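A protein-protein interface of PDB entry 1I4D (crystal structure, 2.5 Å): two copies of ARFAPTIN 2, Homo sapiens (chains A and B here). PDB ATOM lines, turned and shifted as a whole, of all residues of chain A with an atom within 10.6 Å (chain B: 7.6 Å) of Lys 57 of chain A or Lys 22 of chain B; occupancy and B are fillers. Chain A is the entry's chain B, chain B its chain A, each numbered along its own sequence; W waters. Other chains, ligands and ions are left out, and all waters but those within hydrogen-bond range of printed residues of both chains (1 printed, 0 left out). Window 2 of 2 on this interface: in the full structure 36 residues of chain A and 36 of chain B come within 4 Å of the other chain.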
ATOM      1  N   ALA A  46      17.891 -20.497  -8.233  1.00  0.00           N
ATOM      2  CA  ALA A  46      18.755 -21.512  -7.638  1.00  0.00           C
ATOM      3  C   ALA A  46      19.334 -22.453  -8.682  1.00  0.00           C
ATOM      4  O   ALA A  46      20.538 -22.726  -8.701  1.00  0.00           O
ATOM      5  CB  ALA A  46      17.980 -22.309  -6.613  1.00  0.00           C
ATOM      6  N   LEU A  47      18.464 -22.965  -9.539  1.00  0.00           N
ATOM      7  CA  LEU A  47      18.870 -23.883 -10.590  1.00  0.00           C
ATOM      8  C   LEU A  47      19.857 -23.165 -11.492  1.00  0.00           C
ATOM      9  O   LEU A  47      20.772 -23.769 -12.056  1.00  0.00           O
ATOM     10  CB  LEU A  47      17.638 -24.310 -11.386  1.00  0.00           C
ATOM     11  CG  LEU A  47      17.825 -25.397 -12.432  1.00  0.00           C
ATOM     12  CD1 LEU A  47      18.358 -26.655 -11.770  1.00  0.00           C
ATOM     13  CD2 LEU A  47      16.494 -25.670 -13.101  1.00  0.00           C
ATOM     14  N   ASP A  49      22.100 -20.855 -10.616  1.00  0.00           N
ATOM     15  CA  ASP A  49      23.442 -20.816 -10.053  1.00  0.00           C
ATOM     16  C   ASP A  49      24.065 -22.200 -10.164  1.00  0.00           C
ATOM     17  O   ASP A  49      25.194 -22.347 -10.638  1.00  0.00           O
ATOM     18  CB  ASP A  49      23.414 -20.377  -8.586  1.00  0.00           C
ATOM     19  CG  ASP A  49      23.051 -18.917  -8.427  1.00  0.00           C
ATOM     20  OD1 ASP A  49      23.143 -18.390  -7.298  1.00  0.00           O
ATOM     21  OD2 ASP A  49      22.667 -18.292  -9.439  1.00  0.00           O
ATOM     22  N   ALA A  50      23.315 -23.213  -9.738  1.00  0.00           N
ATOM     23  CA  ALA A  50      23.790 -24.587  -9.786  1.00  0.00           C
ATOM     24  C   ALA A  50      24.372 -24.936 -11.152  1.00  0.00           C
ATOM     25  O   ALA A  50      25.477 -25.468 -11.245  1.00  0.00           O
ATOM     26  CB  ALA A  50      22.652 -25.533  -9.444  1.00  0.00           C
ATOM     27  N   PHE A  51      23.627 -24.635 -12.207  1.00  0.00           N
ATOM     28  CA  PHE A  51      24.072 -24.921 -13.558  1.00  0.00           C
ATOM     29  C   PHE A  51      25.291 -24.104 -13.911  1.00  0.00           C
ATOM     30  O   PHE A  51      26.148 -24.557 -14.666  1.00  0.00           O
ATOM     31  CB  PHE A  51      22.964 -24.610 -14.553  1.00  0.00           C
ATOM     32  CG  PHE A  51      21.936 -25.694 -14.678  1.00  0.00           C
ATOM     33  CD1 PHE A  51      20.637 -25.391 -15.065  1.00  0.00           C
ATOM     34  CD2 PHE A  51      22.277 -27.024 -14.465  1.00  0.00           C
ATOM     35  CE1 PHE A  51      19.696 -26.388 -15.242  1.00  0.00           C
ATOM     36  CE2 PHE A  51      21.342 -28.029 -14.641  1.00  0.00           C
ATOM     37  CZ  PHE A  51      20.046 -27.705 -15.032  1.00  0.00           C
ATOM     38  N   ALA A  52      25.357 -22.889 -13.374  1.00  0.00           N
ATOM     39  CA  ALA A  52      26.482 -21.987 -13.630  1.00  0.00           C
ATOM     40  C   ALA A  52      27.733 -22.521 -12.943  1.00  0.00           C
ATOM     41  O   ALA A  52      28.814 -22.524 -13.519  1.00  0.00           O
ATOM     42  CB  ALA A  52      26.159 -20.588 -13.126  1.00  0.00           C
ATOM     43  N   ASP A  53      27.571 -22.978 -11.709  1.00  0.00           N
ATOM     44  CA  ASP A  53      28.674 -23.537 -10.946  1.00  0.00           C
ATOM     45  C   ASP A  53      29.178 -24.797 -11.650  1.00  0.00           C
ATOM     46  O   ASP A  53      30.373 -24.944 -11.882  1.00  0.00           O
ATOM     47  CB  ASP A  53      28.201 -23.864  -9.528  1.00  0.00           C
ATOM     48  CG  ASP A  53      29.280 -24.504  -8.680  1.00  0.00           C
ATOM     49  OD1 ASP A  53      30.395 -23.940  -8.610  1.00  0.00           O
ATOM     50  OD2 ASP A  53      29.003 -25.565  -8.073  1.00  0.00           O
ATOM     51  N   LEU A  54      28.270 -25.703 -11.997  1.00  0.00           N
ATOM     52  CA  LEU A  54      28.661 -26.927 -12.689  1.00  0.00           C
ATOM     53  C   LEU A  54      29.421 -26.595 -13.970  1.00  0.00           C
ATOM     54  O   LEU A  54      30.554 -27.029 -14.150  1.00  0.00           O
ATOM     55  CB  LEU A  54      27.431 -27.778 -13.026  1.00  0.00           C
ATOM     56  CG  LEU A  54      26.871 -28.731 -11.961  1.00  0.00           C
ATOM     57  CD1 LEU A  54      27.824 -29.888 -11.752  1.00  0.00           C
ATOM     58  CD2 LEU A  54      26.646 -27.983 -10.656  1.00  0.00           C
ATOM     59  N   SER A  55      28.796 -25.823 -14.851  1.00  0.00           N
ATOM     60  CA  SER A  55      29.416 -25.439 -16.117  1.00  0.00           C
ATOM     61  C   SER A  55      30.836 -24.901 -15.954  1.00  0.00           C
ATOM     62  O   SER A  55      31.718 -25.175 -16.771  1.00  0.00           O
ATOM     63  CB  SER A  55      28.566 -24.382 -16.817  1.00  0.00           C
ATOM     64  OG  SER A  55      29.201 -23.942 -18.000  1.00  0.00           O
ATOM     65  N   GLN A  56      31.052 -24.128 -14.900  1.00  0.00           N
ATOM     66  CA  GLN A  56      32.365 -23.554 -14.635  1.00  0.00           C
ATOM     67  C   GLN A  56      33.359 -24.613 -14.173  1.00  0.00           C
ATOM     68  O   GLN A  56      34.564 -24.460 -14.358  1.00  0.00           O
ATOM     69  CB  GLN A  56      32.250 -22.444 -13.577  1.00  0.00           C
ATOM     70  CG  GLN A  56      33.584 -21.861 -13.097  1.00  0.00           C
ATOM     71  CD  GLN A  56      33.422 -20.580 -12.265  1.00  0.00           C
ATOM     72  OE1 GLN A  56      32.658 -20.544 -11.292  1.00  0.00           O
ATOM     73  NE2 GLN A  56      34.152 -19.522 -12.646  1.00  0.00           N
ATOM     74  N   LYS A  57      32.854 -25.691 -13.587  1.00  0.00           N
ATOM     75  CA  LYS A  57      33.716 -26.750 -13.081  1.00  0.00           C
ATOM     76  C   LYS A  57      33.501 -28.091 -13.767  1.00  0.00           C
ATOM     77  O   LYS A  57      33.670 -29.145 -13.154  1.00  0.00           O
ATOM     78  CB  LYS A  57      33.492 -26.923 -11.581  1.00  0.00           C
ATOM     79  CG  LYS A  57      33.878 -25.732 -10.742  1.00  0.00           C
ATOM     80  CD  LYS A  57      33.555 -26.006  -9.285  1.00  0.00           C
ATOM     81  CE  LYS A  57      34.136 -24.950  -8.362  1.00  0.00           C
ATOM     82  NZ  LYS A  57      34.031 -25.393  -6.941  1.00  0.00           N
ATOM     83  N   SER A  58      33.133 -28.068 -15.036  1.00  0.00           N
ATOM     84  CA  SER A  58      32.900 -29.314 -15.751  1.00  0.00           C
ATOM     85  C   SER A  58      33.158 -29.069 -17.230  1.00  0.00           C
ATOM     86  O   SER A  58      32.237 -29.056 -18.042  1.00  0.00           O
ATOM     87  CB  SER A  58      31.459 -29.779 -15.518  1.00  0.00           C
ATOM     88  OG  SER A  58      31.232 -31.078 -16.039  1.00  0.00           O
ATOM     89  N   PRO A  59      34.428 -28.861 -17.596  1.00  0.00           N
ATOM     90  CA  PRO A  59      34.794 -28.611 -18.991  1.00  0.00           C
ATOM     91  C   PRO A  59      34.208 -29.616 -19.982  1.00  0.00           C
ATOM     92  O   PRO A  59      34.092 -29.333 -21.176  1.00  0.00           O
ATOM     93  CB  PRO A  59      36.322 -28.633 -18.953  1.00  0.00           C
ATOM     94  CG  PRO A  59      36.639 -29.458 -17.723  1.00  0.00           C
ATOM     95  CD  PRO A  59      35.627 -28.959 -16.749  1.00  0.00           C
ATOM     96  N   GLU A  60      33.819 -30.782 -19.488  1.00  0.00           N
ATOM     97  CA  GLU A  60      33.253 -31.800 -20.360  1.00  0.00           C
ATOM     98  C   GLU A  60      31.929 -31.340 -20.960  1.00  0.00           C
ATOM     99  O   GLU A  60      31.676 -31.505 -22.154  1.00  0.00           O
ATOM    100  CB  GLU A  60      33.021 -33.096 -19.580  1.00  0.00           C
ATOM    101  CG  GLU A  60      34.172 -33.482 -18.666  1.00  0.00           C
ATOM    102  CD  GLU A  60      34.121 -32.771 -17.328  1.00  0.00           C
ATOM    103  OE1 GLU A  60      33.262 -33.138 -16.491  1.00  0.00           O
ATOM    104  OE2 GLU A  60      34.936 -31.844 -17.120  1.00  0.00           O
ATOM    105  N   LEU A  61      31.092 -30.753 -20.111  1.00  0.00           N
ATOM    106  CA  LEU A  61      29.769 -30.285 -20.497  1.00  0.00           C
ATOM    107  C   LEU A  61      29.636 -28.762 -20.398  1.00  0.00           C
ATOM    108  O   LEU A  61      28.535 -28.217 -20.493  1.00  0.00           O
ATOM    109  CB  LEU A  61      28.729 -30.959 -19.596  1.00  0.00           C
ATOM    110  CG  LEU A  61      28.697 -32.492 -19.608  1.00  0.00           C
ATOM    111  CD1 LEU A  61      28.352 -33.013 -18.226  1.00  0.00           C
ATOM    112  CD2 LEU A  61      27.699 -32.979 -20.647  1.00  0.00           C
ATOM    113  N   GLN A  62      30.763 -28.085 -20.207  1.00  0.00           N
ATOM    114  CA  GLN A  62      30.805 -26.631 -20.083  1.00  0.00           C
ATOM    115  C   GLN A  62      29.706 -25.907 -20.861  1.00  0.00           C
ATOM    116  O   GLN A  62      28.990 -25.070 -20.311  1.00  0.00           O
ATOM    117  CB  GLN A  62      32.166 -26.124 -20.547  1.00  0.00           C
ATOM    118  CG  GLN A  62      32.449 -24.682 -20.203  1.00  0.00           C
ATOM    119  CD  GLN A  62      33.814 -24.234 -20.694  1.00  0.00           C
ATOM    120  OE1 GLN A  62      34.010 -23.983 -21.889  1.00  0.00           O
ATOM    121  NE2 GLN A  62      34.773 -24.147 -19.772  1.00  0.00           N
ATOM    122  N   GLU A  63      29.574 -26.223 -22.142  1.00  0.00           N
ATOM    123  CA  GLU A  63      28.561 -25.578 -22.963  1.00  0.00           C
ATOM    124  C   GLU A  63      27.125 -25.871 -22.537  1.00  0.00           C
ATOM    125  O   GLU A  63      26.452 -24.992 -22.002  1.00  0.00           O
ATOM    126  CB  GLU A  63      28.750 -25.965 -24.425  1.00  0.00           C
ATOM    127  CG  GLU A  63      29.748 -25.102 -25.168  1.00  0.00           C
ATOM    128  CD  GLU A  63      29.951 -25.569 -26.601  1.00  0.00           C
ATOM    129  OE1 GLU A  63      28.940 -25.905 -27.262  1.00  0.00           O
ATOM    130  OE2 GLU A  63      31.116 -25.595 -27.067  1.00  0.00           O
ATOM    131  N   PHE A  65      25.853 -27.110 -20.096  1.00  0.00           N
ATOM    132  CA  PHE A  65      25.581 -26.702 -18.729  1.00  0.00           C
ATOM    133  C   PHE A  65      25.494 -25.190 -18.737  1.00  0.00           C
ATOM    134  O   PHE A  65      24.715 -24.599 -17.999  1.00  0.00           O
ATOM    135  CB  PHE A  65      26.708 -27.142 -17.795  1.00  0.00           C
ATOM    136  CG  PHE A  65      26.330 -28.269 -16.879  1.00  0.00           C
ATOM    137  CD1 PHE A  65      27.305 -28.950 -16.165  1.00  0.00           C
ATOM    138  CD2 PHE A  65      25.002 -28.644 -16.723  1.00  0.00           C
ATOM    139  CE1 PHE A  65      26.960 -29.986 -15.315  1.00  0.00           C
ATOM    140  CE2 PHE A  65      24.652 -29.676 -15.873  1.00  0.00           C
ATOM    141  CZ  PHE A  65      25.630 -30.348 -15.168  1.00  0.00           C
ATOM    142  N   GLY A  66      26.299 -24.576 -19.593  1.00  0.00           N
ATOM    143  CA  GLY A  66      26.326 -23.131 -19.696  1.00  0.00           C
ATOM    144  C   GLY A  66      25.060 -22.458 -20.199  1.00  0.00           C
ATOM    145  O   GLY A  66      24.485 -21.624 -19.495  1.00  0.00           O
ATOM    146  N   ALA A  69      22.172 -22.593 -17.948  1.00  0.00           N
ATOM    147  CA  ALA A  69      22.313 -21.673 -16.817  1.00  0.00           C
ATOM    148  C   ALA A  69      21.845 -20.272 -17.184  1.00  0.00           C
ATOM    149  O   ALA A  69      21.165 -19.613 -16.398  1.00  0.00           O
ATOM    150  CB  ALA A  69      23.754 -21.628 -16.346  1.00  0.00           C
ATOM    151  N   LEU B  15      36.612 -35.946  -6.302  1.00  0.00           N
ATOM    152  CA  LEU B  15      36.017 -35.186  -7.381  1.00  0.00           C
ATOM    153  C   LEU B  15      34.663 -35.801  -7.714  1.00  0.00           C
ATOM    154  O   LEU B  15      33.674 -35.091  -7.898  1.00  0.00           O
ATOM    155  CB  LEU B  15      36.921 -35.238  -8.606  1.00  0.00           C
ATOM    156  CG  LEU B  15      36.647 -34.163  -9.651  1.00  0.00           C
ATOM    157  CD1 LEU B  15      37.684 -33.072  -9.451  1.00  0.00           C
ATOM    158  CD2 LEU B  15      36.731 -34.728 -11.074  1.00  0.00           C
ATOM    159  N   LEU B  16      34.621 -37.126  -7.804  1.00  0.00           N
ATOM    160  CA  LEU B  16      33.373 -37.809  -8.108  1.00  0.00           C
ATOM    161  C   LEU B  16      32.423 -37.518  -6.979  1.00  0.00           C
ATOM    162  O   LEU B  16      31.225 -37.336  -7.187  1.00  0.00           O
ATOM    163  CB  LEU B  16      33.575 -39.324  -8.202  1.00  0.00           C
ATOM    164  CG  LEU B  16      32.307 -40.190  -8.220  1.00  0.00           C
ATOM    165  CD1 LEU B  16      31.407 -39.785  -9.370  1.00  0.00           C
ATOM    166  CD2 LEU B  16      32.683 -41.647  -8.364  1.00  0.00           C
ATOM    167  N   ARG B  17      32.963 -37.465  -5.775  1.00  0.00           N
ATOM    168  CA  ARG B  17      32.121 -37.208  -4.627  1.00  0.00           C
ATOM    169  C   ARG B  17      31.451 -35.846  -4.687  1.00  0.00           C
ATOM    170  O   ARG B  17      30.290 -35.717  -4.305  1.00  0.00           O
ATOM    171  CB  ARG B  17      32.922 -37.389  -3.335  1.00  0.00           C
ATOM    172  CG  ARG B  17      32.742 -38.780  -2.735  1.00  0.00           C
ATOM    173  CD  ARG B  17      33.934 -39.229  -1.930  1.00  0.00           C
ATOM    174  NE  ARG B  17      33.688 -40.530  -1.316  1.00  0.00           N
ATOM    175  CZ  ARG B  17      34.646 -41.346  -0.887  1.00  0.00           C
ATOM    176  NH1 ARG B  17      35.926 -40.998  -1.005  1.00  0.00           N
ATOM    177  NH2 ARG B  17      34.325 -42.510  -0.342  1.00  0.00           N
ATOM    178  N   GLU B  18      32.155 -34.830  -5.177  1.00  0.00           N
ATOM    179  CA  GLU B  18      31.527 -33.524  -5.257  1.00  0.00           C
ATOM    180  C   GLU B  18      30.530 -33.543  -6.411  1.00  0.00           C
ATOM    181  O   GLU B  18      29.360 -33.214  -6.223  1.00  0.00           O
ATOM    182  CB  GLU B  18      32.553 -32.394  -5.435  1.00  0.00           C
ATOM    183  CG  GLU B  18      31.971 -31.018  -5.039  1.00  0.00           C
ATOM    184  CD  GLU B  18      32.947 -29.847  -5.207  1.00  0.00           C
ATOM    185  OE1 GLU B  18      33.732 -29.855  -6.185  1.00  0.00           O
ATOM    186  OE2 GLU B  18      32.916 -28.901  -4.373  1.00  0.00           O
ATOM    187  N   THR B  19      30.970 -33.939  -7.600  1.00  0.00           N
ATOM    188  CA  THR B  19      30.054 -34.008  -8.733  1.00  0.00           C
ATOM    189  C   THR B  19      28.759 -34.643  -8.247  1.00  0.00           C
ATOM    190  O   THR B  19      27.674 -34.247  -8.643  1.00  0.00           O
ATOM    191  CB  THR B  19      30.630 -34.866  -9.866  1.00  0.00           C
ATOM    192  OG1 THR B  19      31.703 -34.160 -10.500  1.00  0.00           O
ATOM    193  CG2 THR B  19      29.560 -35.189 -10.893  1.00  0.00           C
ATOM    194  N   LYS B  20      28.889 -35.629  -7.369  1.00  0.00           N
ATOM    195  CA  LYS B  20      27.736 -36.319  -6.810  1.00  0.00           C
ATOM    196  C   LYS B  20      26.822 -35.363  -6.055  1.00  0.00           C
ATOM    197  O   LYS B  20      25.627 -35.303  -6.321  1.00  0.00           O
ATOM    198  CB  LYS B  20      28.196 -37.420  -5.857  1.00  0.00           C
ATOM    199  CG  LYS B  20      27.073 -38.076  -5.062  1.00  0.00           C
ATOM    200  CD  LYS B  20      26.366 -39.162  -5.859  1.00  0.00           C
ATOM    201  CE  LYS B  20      25.167 -39.732  -5.093  1.00  0.00           C
ATOM    202  NZ  LYS B  20      25.488 -40.322  -3.764  1.00  0.00           N
ATOM    203  N   ARG B  21      27.383 -34.628  -5.101  1.00  0.00           N
ATOM    204  CA  ARG B  21      26.601 -33.679  -4.313  1.00  0.00           C
ATOM    205  C   ARG B  21      25.866 -32.664  -5.188  1.00  0.00           C
ATOM    206  O   ARG B  21      24.644 -32.514  -5.098  1.00  0.00           O
ATOM    207  CB  ARG B  21      27.512 -32.941  -3.324  1.00  0.00           C
ATOM    208  CG  ARG B  21      27.734 -33.674  -2.017  1.00  0.00           C
ATOM    209  CD  ARG B  21      28.912 -33.096  -1.256  1.00  0.00           C
ATOM    210  NE  ARG B  21      30.181 -33.401  -1.918  1.00  0.00           N
ATOM    211  CZ  ARG B  21      31.382 -33.122  -1.416  1.00  0.00           C
ATOM    212  NH1 ARG B  21      31.489 -32.524  -0.236  1.00  0.00           N
ATOM    213  NH2 ARG B  21      32.477 -33.445  -2.092  1.00  0.00           N
ATOM    214  N   LYS B  22      26.626 -31.965  -6.024  1.00  0.00           N
ATOM    215  CA  LYS B  22      26.076 -30.969  -6.921  1.00  0.00           C
ATOM    216  C   LYS B  22      24.918 -31.525  -7.721  1.00  0.00           C
ATOM    217  O   LYS B  22      23.882 -30.886  -7.864  1.00  0.00           O
ATOM    218  CB  LYS B  22      27.172 -30.465  -7.848  1.00  0.00           C
ATOM    219  CG  LYS B  22      28.236 -29.701  -7.093  1.00  0.00           C
ATOM    220  CD  LYS B  22      29.306 -29.108  -7.994  1.00  0.00           C
ATOM    221  CE  LYS B  22      30.395 -28.472  -7.131  1.00  0.00           C
ATOM    222  NZ  LYS B  22      31.520 -27.908  -7.927  1.00  0.00           N
ATOM    223  N   TYR B  23      25.090 -32.726  -8.239  1.00  0.00           N
ATOM    224  CA  TYR B  23      24.030 -33.352  -9.009  1.00  0.00           C
ATOM    225  C   TYR B  23      22.790 -33.586  -8.158  1.00  0.00           C
ATOM    226  O   TYR B  23      21.671 -33.395  -8.624  1.00  0.00           O
ATOM    227  CB  TYR B  23      24.520 -34.670  -9.608  1.00  0.00           C
ATOM    228  CG  TYR B  23      25.221 -34.486 -10.924  1.00  0.00           C
ATOM    229  CD1 TYR B  23      26.279 -33.589 -11.052  1.00  0.00           C
ATOM    230  CD2 TYR B  23      24.833 -35.207 -12.045  1.00  0.00           C
ATOM    231  CE1 TYR B  23      26.937 -33.415 -12.268  1.00  0.00           C
ATOM    232  CE2 TYR B  23      25.481 -35.043 -13.272  1.00  0.00           C
ATOM    233  CZ  TYR B  23      26.534 -34.149 -13.377  1.00  0.00           C
ATOM    234  OH  TYR B  23      27.195 -34.006 -14.578  1.00  0.00           O
ATOM    235  N   GLU B  24      22.983 -33.994  -6.911  1.00  0.00           N
ATOM    236  CA  GLU B  24      21.846 -34.240  -6.041  1.00  0.00           C
ATOM    237  C   GLU B  24      21.156 -32.923  -5.711  1.00  0.00           C
ATOM    238  O   GLU B  24      20.010 -32.907  -5.237  1.00  0.00           O
ATOM    239  CB  GLU B  24      22.289 -34.946  -4.761  1.00  0.00           C
ATOM    240  CG  GLU B  24      22.914 -36.306  -5.011  1.00  0.00           C
ATOM    241  CD  GLU B  24      23.295 -37.042  -3.731  1.00  0.00           C
ATOM    242  OE1 GLU B  24      23.932 -36.415  -2.849  1.00  0.00           O
ATOM    243  OE2 GLU B  24      22.966 -38.253  -3.618  1.00  0.00           O
ATOM    244  N   SER B  25      21.856 -31.816  -5.958  1.00  0.00           N
ATOM    245  CA  SER B  25      21.281 -30.498  -5.704  1.00  0.00           C
ATOM    246  C   SER B  25      20.463 -30.087  -6.918  1.00  0.00           C
ATOM    247  O   SER B  25      19.360 -29.567  -6.783  1.00  0.00           O
ATOM    248  CB  SER B  25      22.367 -29.466  -5.444  1.00  0.00           C
ATOM    249  OG  SER B  25      21.788 -28.176  -5.382  1.00  0.00           O
ATOM    250  N   VAL B  26      21.017 -30.300  -8.106  1.00  0.00           N
ATOM    251  CA  VAL B  26      20.290 -30.007  -9.329  1.00  0.00           C
ATOM    252  C   VAL B  26      19.047 -30.880  -9.210  1.00  0.00           C
ATOM    253  O   VAL B  26      17.942 -30.494  -9.587  1.00  0.00           O
ATOM    254  CB  VAL B  26      21.082 -30.444 -10.570  1.00  0.00           C
ATOM    255  CG1 VAL B  26      20.148 -30.603 -11.752  1.00  0.00           C
ATOM    256  CG2 VAL B  26      22.143 -29.418 -10.892  1.00  0.00           C
ATOM    257  N   LEU B  27      19.243 -32.062  -8.642  1.00  0.00           N
ATOM    258  CA  LEU B  27      18.170 -33.014  -8.452  1.00  0.00           C
ATOM    259  C   LEU B  27      17.044 -32.453  -7.570  1.00  0.00           C
ATOM    260  O   LEU B  27      15.874 -32.712  -7.832  1.00  0.00           O
ATOM    261  CB  LEU B  27      18.753 -34.293  -7.860  1.00  0.00           C
ATOM    262  CG  LEU B  27      18.272 -35.640  -8.399  1.00  0.00           C
ATOM    263  CD1 LEU B  27      17.823 -35.533  -9.849  1.00  0.00           C
ATOM    264  CD2 LEU B  27      19.415 -36.633  -8.259  1.00  0.00           C
ATOM    265  N   GLN B  28      17.391 -31.697  -6.525  1.00  0.00           N
ATOM    266  CA  GLN B  28      16.379 -31.090  -5.635  1.00  0.00           C
ATOM    267  C   GLN B  28      15.541 -30.166  -6.492  1.00  0.00           C
ATOM    268  O   GLN B  28      14.383 -30.443  -6.815  1.00  0.00           O
ATOM    269  CB  GLN B  28      17.026 -30.218  -4.553  1.00  0.00           C
ATOM    270  CG  GLN B  28      17.531 -30.923  -3.311  1.00  0.00           C
ATOM    271  CD  GLN B  28      16.419 -31.297  -2.341  1.00  0.00           C
ATOM    272  OE1 GLN B  28      15.617 -32.204  -2.614  1.00  0.00           O
ATOM    273  NE2 GLN B  28      16.363 -30.601  -1.200  1.00  0.00           N
ATOM    274  N   LEU B  29      16.167 -29.045  -6.834  1.00  0.00           N
ATOM    275  CA  LEU B  29      15.568 -28.025  -7.659  1.00  0.00           C
ATOM    276  C   LEU B  29      14.696 -28.663  -8.721  1.00  0.00           C
ATOM    277  O   LEU B  29      13.536 -28.312  -8.865  1.00  0.00           O
ATOM    278  CB  LEU B  29      16.677 -27.206  -8.305  1.00  0.00           C
ATOM    279  CG  LEU B  29      17.694 -26.705  -7.280  1.00  0.00           C
ATOM    280  CD1 LEU B  29      18.714 -25.814  -7.969  1.00  0.00           C
ATOM    281  CD2 LEU B  29      16.973 -25.947  -6.174  1.00  0.00           C
ATOM    282  N   VAL B  97      22.599 -40.793 -10.774  1.00  0.00           N
ATOM    283  CA  VAL B  97      23.121 -40.480  -9.448  1.00  0.00           C
ATOM    284  C   VAL B  97      22.874 -41.522  -8.385  1.00  0.00           C
ATOM    285  O   VAL B  97      23.736 -41.767  -7.548  1.00  0.00           O
ATOM    286  CB  VAL B  97      22.536 -39.165  -8.922  1.00  0.00           C
ATOM    287  CG1 VAL B  97      23.055 -38.899  -7.517  1.00  0.00           C
ATOM    288  CG2 VAL B  97      22.884 -38.024  -9.869  1.00  0.00           C
ATOM    289  N   LYS B 173      28.454 -40.429 -17.635  1.00  0.00           N
ATOM    290  CA  LYS B 173      28.003 -39.172 -17.055  1.00  0.00           C
ATOM    291  C   LYS B 173      27.712 -38.194 -18.189  1.00  0.00           C
ATOM    292  O   LYS B 173      26.649 -37.573 -18.236  1.00  0.00           O
ATOM    293  CB  LYS B 173      29.077 -38.580 -16.145  1.00  0.00           C
ATOM    294  CG  LYS B 173      28.563 -37.446 -15.288  1.00  0.00           C
ATOM    295  CD  LYS B 173      29.643 -36.835 -14.420  1.00  0.00           C
ATOM    296  CE  LYS B 173      30.535 -35.885 -15.206  1.00  0.00           C
ATOM    297  NZ  LYS B 173      31.511 -35.194 -14.303  1.00  0.00           N
HETATM  298  O   HOH W   1      31.853 -31.521 -11.347  1.00  0.00           O
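Of the 20 printed residues of chain A, 7 touch a printed residue of chain B. Hydrophobic or aromatic side chains of chain A within 4 Å of the printed part of chain B: Ala 46, Leu 47, Leu 54 and Leu 61. Among the printed residues, 8 pairs touch across the chains. Among the printed residues, Asp or Glu carboxylates within 4 Å of a Lys or Arg side-chain nitrogen of the other chain: Asp 53 of chain A with Lys 22 of chain B and Glu 60 of chain A with Lys 173 of chain B.
Among the printed residues, merely in contact across the chains: Lys 57 of chain A with Lys 22 of chain B, Leu 47 of chain A with Leu 29 of chain B, Ala 46 of chain A with Leu 29 of chain B, Leu 54 of chain A with Tyr 23 of chain B, Leu 54 of chain A with Lys 22 of chain B and Leu 61 of chain A with Tyr 23 of chain B.
No position is printed for both chains. Of the 8 pairs that touch across the chains among the printed residues, none has its exchanged pair printed and touching as well.
NZ of Lys 22 of chain B is in salt-bridge range of OD2 of Asp 53 of chain A (3.4 Å). OE1 of Glu 60 of chain A is in salt-bridge range of NZ of Lys 173 of chain B (3.5 Å).
Lys 57 of chain A touches just one residue of chain B: Lys 22 (3.1 Å). Lys 22 of chain B touches three residues of chain A. No residue of chain A comes within 4 Å of Glu 18 of chain B. No residue of chain A comes within 4 Å of Ser 25 of chain B. No residue of chain A comes within 4 Å of Val 26 of chain B. Printed residues of chain A within 4 Å of Leu 29 of chain B: Ala 46 (3.5 Å) and Leu 47 (3.3 Å). Of the printed residues of chain A, Tyr 23 of chain B touches Leu 54 (3.7 Å) and Leu 61 (3.95 Å). Printed residues of chain B within 4 Å of Glu 60 of chain A: Lys 173. Printed residues of chain B within 4 Å of Leu 54 of chain A: Lys 22 (3.8 Å) and Tyr 23 (3.7 Å). Leu 16 of chain B touches none of the printed residues of chain A. Gly 66 of chain A touches none of the printed residues of chain B. The nearest residue of chain B that does not touch Lys 57 of chain A is Glu 18 of chain B (4.5 Å). The nearest printed residue of chain A that does not touch Leu 29 of chain B is Ala 50 of chain A (4.2 Å).
The side-chain hydroxyl (OG) of Ser 58 of chain A sits at hydrogen-bond distance from the side-chain carboxylate (OE1) of Glu 60 of chain A (2.9 Å). The side-chain amino group of Lys 22 of chain B lies within salt-bridge range of the side-chain carboxylate of Glu 18 of chain B, 3.4 Å away.
Water W1 bridges the side-chain hydroxyl (OG1) of Thr 19 of chain B and the backbone carbonyl oxygen (O) of Lys 57 of chain A.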
